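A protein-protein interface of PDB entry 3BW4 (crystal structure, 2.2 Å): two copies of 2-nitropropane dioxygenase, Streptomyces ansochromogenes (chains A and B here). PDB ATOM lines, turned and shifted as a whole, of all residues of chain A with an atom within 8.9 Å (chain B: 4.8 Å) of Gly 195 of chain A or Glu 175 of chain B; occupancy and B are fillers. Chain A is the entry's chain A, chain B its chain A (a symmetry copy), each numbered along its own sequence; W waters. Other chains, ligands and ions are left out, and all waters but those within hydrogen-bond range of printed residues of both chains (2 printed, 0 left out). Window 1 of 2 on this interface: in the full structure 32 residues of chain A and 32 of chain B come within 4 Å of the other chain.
The side-chain carboxylate (OE1) of Glu 175 of chain B sits at hydrogen-bond distance from the backbone NH (N) of Leu 196 of chain B (3.0 Å).
The backbone carbonyl oxygen (O) of Ile 194 of chain A sits at hydrogen-bond distance from the backbone NH (N) of Val 174 of chain A.
The side-chain amide nitrogen (NE2) of Gln 202 of chain A lies within hydrogen-bond range of the side-chain hydroxyl (OG) of Ser 198 of chain A (3.3 Å).
The backbone NH (N) of Gln 323 of chain B is in hydrogen-bond range of the backbone carbonyl oxygen (O) of Glu 175 of chain B.
The backbone NH (N) of Gln 323 of chain A is in hydrogen-bond range of the backbone carbonyl oxygen (O) of Glu 175 of chain A (3.0 Å).
The backbone NH of Val 174 of chain B sits at hydrogen-bond distance from the backbone carbonyl oxygen of Ile 194 of chain B (2.9 Å).
N of Gly 195 of chain B lies within hydrogen-bond range of OE1 of Gln 323 of chain A (2.9 Å).
The side-chain amide oxygen (OE1) of Gln 323 of chain B sits at hydrogen-bond distance from the backbone NH (N) of Gly 195 of chain A (2.9 Å).
The backbone carbonyl oxygen (O) of Gly 193 of chain A lies within hydrogen-bond range of the side-chain amide nitrogen (NE2) of Gln 323 of chain B (2.8 Å).
NE2 of Gln 202 of chain A is in hydrogen-bond range of O of Gln 323 of chain B, at 3.3 Å.
Water W2 lies within hydrogen-bond range of OG of Ser 198 of chain A (2.6 Å) and O of Gly 216 of chain B (2.6 Å).
Water W1 lies within hydrogen-bond range of the backbone carbonyl oxygen (O) of Gly 215 of chain B, the side-chain carboxylate (OE2) of Glu 175 of chain B and the backbone NH (N) of Ser 198 of chain A.
Among the printed residues, pairs that only touch across the chains: Gly 195 of chain A with Glu 175 of chain B, Glu 175 of chain A with Gly 195 of chain B, Gln 323 of chain A with Ile 194 of chain B, Ile 194 of chain A with Gln 323 of chain B, Ser 198 of chain A with Gln 323 of chain B, Leu 196 of chain A with Leu 197 of chain B and Leu 197 of chain A with Leu 196 of chain B.
Glu 175 of chain A touches Gly 195 of chain B, and with the chains exchanged Gly 195 of chain A touches Glu 175 of chain B.
Ile 194 of chain A touches Gln 323 of chain B, and with the chains exchanged Gln 323 of chain A touches Ile 194 of chain B.
Gly 195 of chain A touches Gln 323 of chain B, and with the chains exchanged Gln 323 of chain A touches Gly 195 of chain B.
Leu 196 of chain A touches Leu 197 of chain B, and with the chains exchanged Leu 197 of chain A touches Leu 196 of chain B.
Positions printed for both chains: 173, 174, 175, 176, 194, 195, 196, 197, 215, 276 and 323.
Printed residues of chain B within 4 Å of Gly 193 of chain A: Gln 323 (2.8 Å).
Of chain B, only Glu 175 and Gln 323 come within 4 Å of Gly 195 of chain A.
Printed residues of chain B within 4 Å of Leu 197 of chain A: Leu 196.
Printed residues of chain B within 4 Å of Ser 198 of chain A: Gln 323.
Of the printed residues of chain B, Gln 202 of chain A touches Gln 323 (3.3 Å).
No residue of chain A comes within 4 Å of Val 174 of chain B.
Glu 175 of chain B touches one residue of chain A.
No residue of chain A comes within 4 Å of Gly 322 of chain B.
The nearest printed residue of chain B that does not touch Gly 195 of chain A is Gly 195 of chain B (4.8 Å).
Along chain B the printed residues that touch a printed residue of chain A span positions 175 to 323.
Hydrophobic or aromatic side chains of chain A within 4 Å of the printed part of chain B: Ile 194, Leu 196 and Leu 197.
Among the printed residues, no Asp or Glu carboxylate lies within 4 Å of a Lys or Arg side-chain nitrogen of the other chain.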
ATOM      1  N   THR A 153       5.795 -13.586  -3.177  1.00  0.00           N
ATOM      2  CA  THR A 153       5.718 -13.206  -1.770  1.00  0.00           C
ATOM      3  C   THR A 153       6.915 -13.725  -0.968  1.00  0.00           C
ATOM      4  O   THR A 153       7.023 -13.473   0.234  1.00  0.00           O
ATOM      5  CB  THR A 153       4.408 -13.727  -1.125  1.00  0.00           C
ATOM      6  OG1 THR A 153       4.421 -15.160  -1.086  1.00  0.00           O
ATOM      7  CG2 THR A 153       3.191 -13.253  -1.933  1.00  0.00           C
ATOM      8  N   ALA A 171       7.217  -7.727  -5.764  1.00  0.00           N
ATOM      9  CA  ALA A 171       7.448  -8.234  -4.416  1.00  0.00           C
ATOM     10  C   ALA A 171       6.332  -7.698  -3.532  1.00  0.00           C
ATOM     11  O   ALA A 171       6.360  -6.540  -3.124  1.00  0.00           O
ATOM     12  CB  ALA A 171       8.809  -7.769  -3.902  1.00  0.00           C
ATOM     13  N   GLN A 172       5.344  -8.540  -3.249  1.00  0.00           N
ATOM     14  CA  GLN A 172       4.211  -8.140  -2.427  1.00  0.00           C
ATOM     15  C   GLN A 172       4.412  -8.565  -0.974  1.00  0.00           C
ATOM     16  O   GLN A 172       4.390  -9.757  -0.661  1.00  0.00           O
ATOM     17  CB  GLN A 172       2.921  -8.757  -2.981  1.00  0.00           C
ATOM     18  CG  GLN A 172       1.662  -8.412  -2.194  1.00  0.00           C
ATOM     19  CD  GLN A 172       0.505  -9.347  -2.514  1.00  0.00           C
ATOM     20  OE1 GLN A 172       0.674 -10.569  -2.533  1.00  0.00           O
ATOM     21  NE2 GLN A 172      -0.679  -8.778  -2.751  1.00  0.00           N
ATOM     22  N   GLY A 173       4.600  -7.580  -0.095  1.00  0.00           N
ATOM     23  CA  GLY A 173       4.809  -7.853   1.319  1.00  0.00           C
ATOM     24  C   GLY A 173       3.534  -8.185   2.077  1.00  0.00           C
ATOM     25  O   GLY A 173       2.427  -8.046   1.553  1.00  0.00           O
ATOM     26  N   VAL A 174       3.687  -8.595   3.330  1.00  0.00           N
ATOM     27  CA  VAL A 174       2.554  -8.986   4.156  1.00  0.00           C
ATOM     28  C   VAL A 174       1.570  -7.851   4.471  1.00  0.00           C
ATOM     29  O   VAL A 174       0.410  -8.113   4.793  1.00  0.00           O
ATOM     30  CB  VAL A 174       3.055  -9.633   5.479  1.00  0.00           C
ATOM     31  CG1 VAL A 174       3.575  -8.558   6.419  1.00  0.00           C
ATOM     32  CG2 VAL A 174       1.950 -10.445   6.124  1.00  0.00           C
ATOM     33  N   GLU A 175       2.026  -6.603   4.366  1.00  0.00           N
ATOM     34  CA  GLU A 175       1.178  -5.439   4.653  1.00  0.00           C
ATOM     35  C   GLU A 175       0.161  -5.137   3.553  1.00  0.00           C
ATOM     36  O   GLU A 175      -0.809  -4.411   3.778  1.00  0.00           O
ATOM     37  CB  GLU A 175       2.027  -4.173   4.847  1.00  0.00           C
ATOM     38  CG  GLU A 175       3.183  -4.301   5.832  1.00  0.00           C
ATOM     39  CD  GLU A 175       4.478  -4.680   5.147  1.00  0.00           C
ATOM     40  OE1 GLU A 175       4.515  -5.736   4.477  1.00  0.00           O
ATOM     41  OE2 GLU A 175       5.455  -3.919   5.275  1.00  0.00           O
ATOM     42  N   ALA A 176       0.399  -5.683   2.366  1.00  0.00           N
ATOM     43  CA  ALA A 176      -0.464  -5.445   1.215  1.00  0.00           C
ATOM     44  C   ALA A 176      -1.945  -5.708   1.467  1.00  0.00           C
ATOM     45  O   ALA A 176      -2.314  -6.569   2.267  1.00  0.00           O
ATOM     46  CB  ALA A 176       0.020  -6.292   0.027  1.00  0.00           C
ATOM     47  N   GLN A 180      -3.088 -12.155  -1.127  1.00  0.00           N
ATOM     48  CA  GLN A 180      -1.655 -12.403  -1.105  1.00  0.00           C
ATOM     49  C   GLN A 180      -1.414 -13.186  -2.387  1.00  0.00           C
ATOM     50  O   GLN A 180      -2.118 -14.158  -2.659  1.00  0.00           O
ATOM     51  CB  GLN A 180      -1.277 -13.250   0.111  1.00  0.00           C
ATOM     52  CG  GLN A 180      -1.126 -12.454   1.400  1.00  0.00           C
ATOM     53  CD  GLN A 180       0.100 -11.555   1.378  1.00  0.00           C
ATOM     54  OE1 GLN A 180      -0.010 -10.327   1.311  1.00  0.00           O
ATOM     55  NE2 GLN A 180       1.280 -12.166   1.426  1.00  0.00           N
ATOM     56  N   ALA A 192       3.144 -16.663   8.231  1.00  0.00           N
ATOM     57  CA  ALA A 192       4.456 -16.713   7.599  1.00  0.00           C
ATOM     58  C   ALA A 192       4.755 -15.511   6.697  1.00  0.00           C
ATOM     59  O   ALA A 192       5.813 -15.448   6.077  1.00  0.00           O
ATOM     60  CB  ALA A 192       4.585 -18.009   6.801  1.00  0.00           C
ATOM     61  N   GLY A 193       3.829 -14.556   6.630  1.00  0.00           N
ATOM     62  CA  GLY A 193       4.027 -13.389   5.782  1.00  0.00           C
ATOM     63  C   GLY A 193       5.284 -12.578   6.053  1.00  0.00           C
ATOM     64  O   GLY A 193       5.625 -12.307   7.203  1.00  0.00           O
ATOM     65  N   ILE A 194       5.966 -12.161   4.994  1.00  0.00           N
ATOM     66  CA  ILE A 194       7.192 -11.383   5.148  1.00  0.00           C
ATOM     67  C   ILE A 194       6.985  -9.870   4.972  1.00  0.00           C
ATOM     68  O   ILE A 194       6.390  -9.422   3.990  1.00  0.00           O
ATOM     69  CB  ILE A 194       8.263 -11.880   4.150  1.00  0.00           C
ATOM     70  CG1 ILE A 194       8.466 -13.391   4.330  1.00  0.00           C
ATOM     71  CG2 ILE A 194       9.585 -11.140   4.377  1.00  0.00           C
ATOM     72  CD1 ILE A 194       9.387 -14.014   3.310  1.00  0.00           C
ATOM     73  N   GLY A 195       7.467  -9.090   5.938  1.00  0.00           N
ATOM     74  CA  GLY A 195       7.342  -7.642   5.852  1.00  0.00           C
ATOM     75  C   GLY A 195       8.005  -7.176   4.572  1.00  0.00           C
ATOM     76  O   GLY A 195       9.082  -7.668   4.223  1.00  0.00           O
ATOM     77  N   LEU A 196       7.377  -6.237   3.869  1.00  0.00           N
ATOM     78  CA  LEU A 196       7.918  -5.745   2.601  1.00  0.00           C
ATOM     79  C   LEU A 196       9.396  -5.363   2.603  1.00  0.00           C
ATOM     80  O   LEU A 196      10.143  -5.772   1.714  1.00  0.00           O
ATOM     81  CB  LEU A 196       7.104  -4.545   2.092  1.00  0.00           C
ATOM     82  CG  LEU A 196       7.548  -3.961   0.741  1.00  0.00           C
ATOM     83  CD1 LEU A 196       7.471  -5.043  -0.351  1.00  0.00           C
ATOM     84  CD2 LEU A 196       6.647  -2.780   0.366  1.00  0.00           C
ATOM     85  N   LEU A 197       9.816  -4.571   3.585  1.00  0.00           N
ATOM     86  CA  LEU A 197      11.206  -4.126   3.640  1.00  0.00           C
ATOM     87  C   LEU A 197      12.175  -5.306   3.658  1.00  0.00           C
ATOM     88  O   LEU A 197      13.263  -5.247   3.078  1.00  0.00           O
ATOM     89  CB  LEU A 197      11.435  -3.234   4.866  1.00  0.00           C
ATOM     90  CG  LEU A 197      12.800  -2.532   4.959  1.00  0.00           C
ATOM     91  CD1 LEU A 197      13.079  -1.736   3.679  1.00  0.00           C
ATOM     92  CD2 LEU A 197      12.810  -1.604   6.167  1.00  0.00           C
ATOM     93  N   SER A 198      11.769  -6.382   4.317  1.00  0.00           N
ATOM     94  CA  SER A 198      12.600  -7.570   4.398  1.00  0.00           C
ATOM     95  C   SER A 198      12.477  -8.361   3.096  1.00  0.00           C
ATOM     96  O   SER A 198      13.479  -8.777   2.518  1.00  0.00           O
ATOM     97  CB  SER A 198      12.171  -8.426   5.588  1.00  0.00           C
ATOM     98  OG  SER A 198      13.141  -9.414   5.869  1.00  0.00           O
ATOM     99  N   LEU A 199      11.247  -8.553   2.626  1.00  0.00           N
ATOM    100  CA  LEU A 199      11.016  -9.286   1.383  1.00  0.00           C
ATOM    101  C   LEU A 199      11.762  -8.652   0.206  1.00  0.00           C
ATOM    102  O   LEU A 199      12.402  -9.350  -0.582  1.00  0.00           O
ATOM    103  CB  LEU A 199       9.520  -9.339   1.059  1.00  0.00           C
ATOM    104  CG  LEU A 199       9.161  -9.968  -0.295  1.00  0.00           C
ATOM    105  CD1 LEU A 199       9.625 -11.424  -0.328  1.00  0.00           C
ATOM    106  CD2 LEU A 199       7.653  -9.877  -0.522  1.00  0.00           C
ATOM    107  N   LEU A 200      11.671  -7.329   0.089  1.00  0.00           N
ATOM    108  CA  LEU A 200      12.340  -6.613  -0.995  1.00  0.00           C
ATOM    109  C   LEU A 200      13.844  -6.881  -1.046  1.00  0.00           C
ATOM    110  O   LEU A 200      14.401  -7.130  -2.116  1.00  0.00           O
ATOM    111  CB  LEU A 200      12.098  -5.108  -0.859  1.00  0.00           C
ATOM    112  CG  LEU A 200      12.832  -4.211  -1.858  1.00  0.00           C
ATOM    113  CD1 LEU A 200      12.451  -4.586  -3.297  1.00  0.00           C
ATOM    114  CD2 LEU A 200      12.482  -2.754  -1.565  1.00  0.00           C
ATOM    115  N   ALA A 201      14.500  -6.826   0.107  1.00  0.00           N
ATOM    116  CA  ALA A 201      15.936  -7.063   0.167  1.00  0.00           C
ATOM    117  C   ALA A 201      16.269  -8.502  -0.225  1.00  0.00           C
ATOM    118  O   ALA A 201      17.269  -8.752  -0.901  1.00  0.00           O
ATOM    119  CB  ALA A 201      16.460  -6.770   1.576  1.00  0.00           C
ATOM    120  N   GLN A 202      15.427  -9.443   0.204  1.00  0.00           N
ATOM    121  CA  GLN A 202      15.644 -10.852  -0.112  1.00  0.00           C
ATOM    122  C   GLN A 202      15.449 -11.115  -1.606  1.00  0.00           C
ATOM    123  O   GLN A 202      16.221 -11.847  -2.224  1.00  0.00           O
ATOM    124  CB  GLN A 202      14.681 -11.737   0.691  1.00  0.00           C
ATOM    125  CG  GLN A 202      14.870 -11.699   2.203  1.00  0.00           C
ATOM    126  CD  GLN A 202      13.893 -12.616   2.926  1.00  0.00           C
ATOM    127  OE1 GLN A 202      13.855 -13.821   2.676  1.00  0.00           O
ATOM    128  NE2 GLN A 202      13.097 -12.049   3.822  1.00  0.00           N
ATOM    129  N   VAL A 203      14.409 -10.520  -2.181  1.00  0.00           N
ATOM    130  CA  VAL A 203      14.125 -10.696  -3.601  1.00  0.00           C
ATOM    131  C   VAL A 203      15.201 -10.030  -4.458  1.00  0.00           C
ATOM    132  O   VAL A 203      15.665 -10.607  -5.438  1.00  0.00           O
ATOM    133  CB  VAL A 203      12.741 -10.116  -3.963  1.00  0.00           C
ATOM    134  CG1 VAL A 203      12.555 -10.105  -5.479  1.00  0.00           C
ATOM    135  CG2 VAL A 203      11.645 -10.945  -3.302  1.00  0.00           C
ATOM    136  N   ALA A 214       5.378  -3.765  -3.433  1.00  0.00           N
ATOM    137  CA  ALA A 214       3.962  -3.592  -3.104  1.00  0.00           C
ATOM    138  C   ALA A 214       3.619  -3.956  -1.657  1.00  0.00           C
ATOM    139  O   ALA A 214       4.064  -4.987  -1.140  1.00  0.00           O
ATOM    140  CB  ALA A 214       3.102  -4.432  -4.050  1.00  0.00           C
ATOM    141  N   GLY A 215       2.810  -3.116  -1.015  1.00  0.00           N
ATOM    142  CA  GLY A 215       2.402  -3.395   0.347  1.00  0.00           C
ATOM    143  C   GLY A 215       2.519  -2.249   1.330  1.00  0.00           C
ATOM    144  O   GLY A 215       3.613  -1.927   1.779  1.00  0.00           O
ATOM    145  N   ARG A 276      -6.056  -9.595   2.839  1.00  0.00           N
ATOM    146  CA  ARG A 276      -6.104  -8.636   3.940  1.00  0.00           C
ATOM    147  C   ARG A 276      -7.297  -7.701   3.798  1.00  0.00           C
ATOM    148  O   ARG A 276      -7.454  -7.004   2.787  1.00  0.00           O
ATOM    149  CB  ARG A 276      -4.820  -7.815   4.003  1.00  0.00           C
ATOM    150  CG  ARG A 276      -4.782  -6.859   5.190  1.00  0.00           C
ATOM    151  CD  ARG A 276      -3.451  -6.145   5.295  1.00  0.00           C
ATOM    152  NE  ARG A 276      -2.373  -7.062   5.642  1.00  0.00           N
ATOM    153  CZ  ARG A 276      -2.188  -7.586   6.853  1.00  0.00           C
ATOM    154  NH1 ARG A 276      -3.009  -7.284   7.852  1.00  0.00           N
ATOM    155  NH2 ARG A 276      -1.175  -8.419   7.065  1.00  0.00           N
ATOM    156  N   GLN A 323      -2.231  -2.364   5.412  1.00  0.00           N
ATOM    157  CA  GLN A 323      -2.045  -1.833   6.758  1.00  0.00           C
ATOM    158  C   GLN A 323      -1.905  -0.311   6.818  1.00  0.00           C
ATOM    159  O   GLN A 323      -1.938   0.277   7.894  1.00  0.00           O
ATOM    160  CB  GLN A 323      -0.845  -2.510   7.425  1.00  0.00           C
ATOM    161  CG  GLN A 323      -1.001  -4.015   7.565  1.00  0.00           C
ATOM    162  CD  GLN A 323       0.122  -4.647   8.362  1.00  0.00           C
ATOM    163  OE1 GLN A 323       1.292  -4.420   8.079  1.00  0.00           O
ATOM    164  NE2 GLN A 323      -0.231  -5.449   9.364  1.00  0.00           N
ATOM    165  N   GLY B 173       8.923  -3.142  13.871  1.00  0.00           N
ATOM    166  CA  GLY B 173       7.981  -3.802  12.979  1.00  0.00           C
ATOM    167  C   GLY B 173       7.820  -5.290  13.245  1.00  0.00           C
ATOM    168  O   GLY B 173       8.568  -5.882  14.024  1.00  0.00           O
ATOM    169  N   VAL B 174       6.857  -5.904  12.568  1.00  0.00           N
ATOM    170  CA  VAL B 174       6.567  -7.318  12.757  1.00  0.00           C
ATOM    171  C   VAL B 174       7.698  -8.266  12.336  1.00  0.00           C
ATOM    172  O   VAL B 174       7.754  -9.406  12.802  1.00  0.00           O
ATOM    173  CB  VAL B 174       5.256  -7.699  12.010  1.00  0.00           C
ATOM    174  CG1 VAL B 174       5.515  -7.786  10.516  1.00  0.00           C
ATOM    175  CG2 VAL B 174       4.695  -8.998  12.552  1.00  0.00           C
ATOM    176  N   GLU B 175       8.600  -7.794  11.474  1.00  0.00           N
ATOM    177  CA  GLU B 175       9.719  -8.614  10.994  1.00  0.00           C
ATOM    178  C   GLU B 175      10.833  -8.795  12.025  1.00  0.00           C
ATOM    179  O   GLU B 175      11.668  -9.691  11.897  1.00  0.00           O
ATOM    180  CB  GLU B 175      10.357  -7.995   9.741  1.00  0.00           C
ATOM    181  CG  GLU B 175       9.389  -7.629   8.622  1.00  0.00           C
ATOM    182  CD  GLU B 175       8.931  -6.190   8.711  1.00  0.00           C
ATOM    183  OE1 GLU B 175       8.365  -5.805   9.758  1.00  0.00           O
ATOM    184  OE2 GLU B 175       9.143  -5.445   7.736  1.00  0.00           O
ATOM    185  N   ALA B 176      10.846  -7.930  13.033  1.00  0.00           N
ATOM    186  CA  ALA B 176      11.874  -7.957  14.067  1.00  0.00           C
ATOM    187  C   ALA B 176      12.076  -9.317  14.726  1.00  0.00           C
ATOM    188  O   ALA B 176      11.141 -10.109  14.855  1.00  0.00           O
ATOM    189  CB  ALA B 176      11.556  -6.900  15.137  1.00  0.00           C
ATOM    190  N   GLY B 177      13.312  -9.581  15.132  1.00  0.00           N
ATOM    191  CA  GLY B 177      13.616 -10.824  15.815  1.00  0.00           C
ATOM    192  C   GLY B 177      13.409 -10.600  17.303  1.00  0.00           C
ATOM    193  O   GLY B 177      13.307  -9.457  17.746  1.00  0.00           O
ATOM    194  N   ILE B 194       2.378  -5.127  12.471  1.00  0.00           N
ATOM    195  CA  ILE B 194       2.503  -4.194  11.356  1.00  0.00           C
ATOM    196  C   ILE B 194       3.888  -4.213  10.692  1.00  0.00           C
ATOM    197  O   ILE B 194       4.916  -4.113  11.367  1.00  0.00           O
ATOM    198  CB  ILE B 194       2.172  -2.760  11.827  1.00  0.00           C
ATOM    199  CG1 ILE B 194       0.786  -2.747  12.489  1.00  0.00           C
ATOM    200  CG2 ILE B 194       2.197  -1.792  10.640  1.00  0.00           C
ATOM    201  CD1 ILE B 194       0.415  -1.425  13.116  1.00  0.00           C
ATOM    202  N   GLY B 195       3.909  -4.356   9.367  1.00  0.00           N
ATOM    203  CA  GLY B 195       5.173  -4.362   8.644  1.00  0.00           C
ATOM    204  C   GLY B 195       5.900  -3.065   8.932  1.00  0.00           C
ATOM    205  O   GLY B 195       5.274  -2.002   8.960  1.00  0.00           O
ATOM    206  N   LEU B 196       7.210  -3.137   9.149  1.00  0.00           N
ATOM    207  CA  LEU B 196       7.998  -1.947   9.471  1.00  0.00           C
ATOM    208  C   LEU B 196       7.779  -0.734   8.572  1.00  0.00           C
ATOM    209  O   LEU B 196       7.585   0.378   9.066  1.00  0.00           O
ATOM    210  CB  LEU B 196       9.498  -2.276   9.491  1.00  0.00           C
ATOM    211  CG  LEU B 196      10.433  -1.112   9.860  1.00  0.00           C
ATOM    212  CD1 LEU B 196      10.080  -0.577  11.258  1.00  0.00           C
ATOM    213  CD2 LEU B 196      11.889  -1.591   9.841  1.00  0.00           C
ATOM    214  N   LEU B 197       7.823  -0.935   7.258  1.00  0.00           N
ATOM    215  CA  LEU B 197       7.665   0.179   6.328  1.00  0.00           C
ATOM    216  C   LEU B 197       6.348   0.919   6.556  1.00  0.00           C
ATOM    217  O   LEU B 197       6.272   2.144   6.415  1.00  0.00           O
ATOM    218  CB  LEU B 197       7.748  -0.317   4.879  1.00  0.00           C
ATOM    219  CG  LEU B 197       7.788   0.762   3.785  1.00  0.00           C
ATOM    220  CD1 LEU B 197       8.921   1.757   4.058  1.00  0.00           C
ATOM    221  CD2 LEU B 197       7.986   0.100   2.428  1.00  0.00           C
ATOM    222  N   GLY B 215      13.619  -3.924  12.721  1.00  0.00           N
ATOM    223  CA  GLY B 215      12.915  -5.055  12.152  1.00  0.00           C
ATOM    224  C   GLY B 215      13.357  -5.494  10.770  1.00  0.00           C
ATOM    225  O   GLY B 215      13.022  -4.853   9.780  1.00  0.00           O
ATOM    226  N   GLY B 216      14.108  -6.591  10.711  1.00  0.00           N
ATOM    227  CA  GLY B 216      14.570  -7.135   9.445  1.00  0.00           C
ATOM    228  C   GLY B 216      15.664  -6.385   8.701  1.00  0.00           C
ATOM    229  O   GLY B 216      15.948  -6.712   7.550  1.00  0.00           O
ATOM    230  N   ARG B 276       9.754 -13.584  17.936  1.00  0.00           N
ATOM    231  CA  ARG B 276      10.048 -14.230  16.661  1.00  0.00           C
ATOM    232  C   ARG B 276      11.301 -15.089  16.759  1.00  0.00           C
ATOM    233  O   ARG B 276      12.386 -14.608  17.109  1.00  0.00           O
ATOM    234  CB  ARG B 276      10.227 -13.195  15.554  1.00  0.00           C
ATOM    235  CG  ARG B 276      10.450 -13.823  14.182  1.00  0.00           C
ATOM    236  CD  ARG B 276      10.507 -12.777  13.088  1.00  0.00           C
ATOM    237  NE  ARG B 276       9.217 -12.130  12.893  1.00  0.00           N
ATOM    238  CZ  ARG B 276       8.170 -12.698  12.296  1.00  0.00           C
ATOM    239  NH1 ARG B 276       8.251 -13.935  11.824  1.00  0.00           N
ATOM    240  NH2 ARG B 276       7.032 -12.023  12.173  1.00  0.00           N
ATOM    241  N   GLY B 322      15.154 -12.267  13.219  1.00  0.00           N
ATOM    242  CA  GLY B 322      14.220 -11.516  12.399  1.00  0.00           C
ATOM    243  C   GLY B 322      14.056 -12.190  11.052  1.00  0.00           C
ATOM    244  O   GLY B 322      14.800 -13.113  10.723  1.00  0.00           O
ATOM    245  N   GLN B 323      13.095 -11.731  10.259  1.00  0.00           N
ATOM    246  CA  GLN B 323      12.844 -12.344   8.958  1.00  0.00           C
ATOM    247  C   GLN B 323      14.006 -12.215   7.971  1.00  0.00           C
ATOM    248  O   GLN B 323      14.004 -12.847   6.921  1.00  0.00           O
ATOM    249  CB  GLN B 323      11.559 -11.775   8.352  1.00  0.00           C
ATOM    250  CG  GLN B 323      10.326 -12.031   9.203  1.00  0.00           C
ATOM    251  CD  GLN B 323       9.045 -11.599   8.517  1.00  0.00           C
ATOM    252  OE1 GLN B 323       8.941 -10.475   8.042  1.00  0.00           O
ATOM    253  NE2 GLN B 323       8.060 -12.493   8.469  1.00  0.00           N
HETATM  254  O   HOH W   1      11.974  -5.401   7.375  1.00  0.00           O
HETATM  255  O   HOH W   2      15.555  -8.487   5.648  1.00  0.00           O
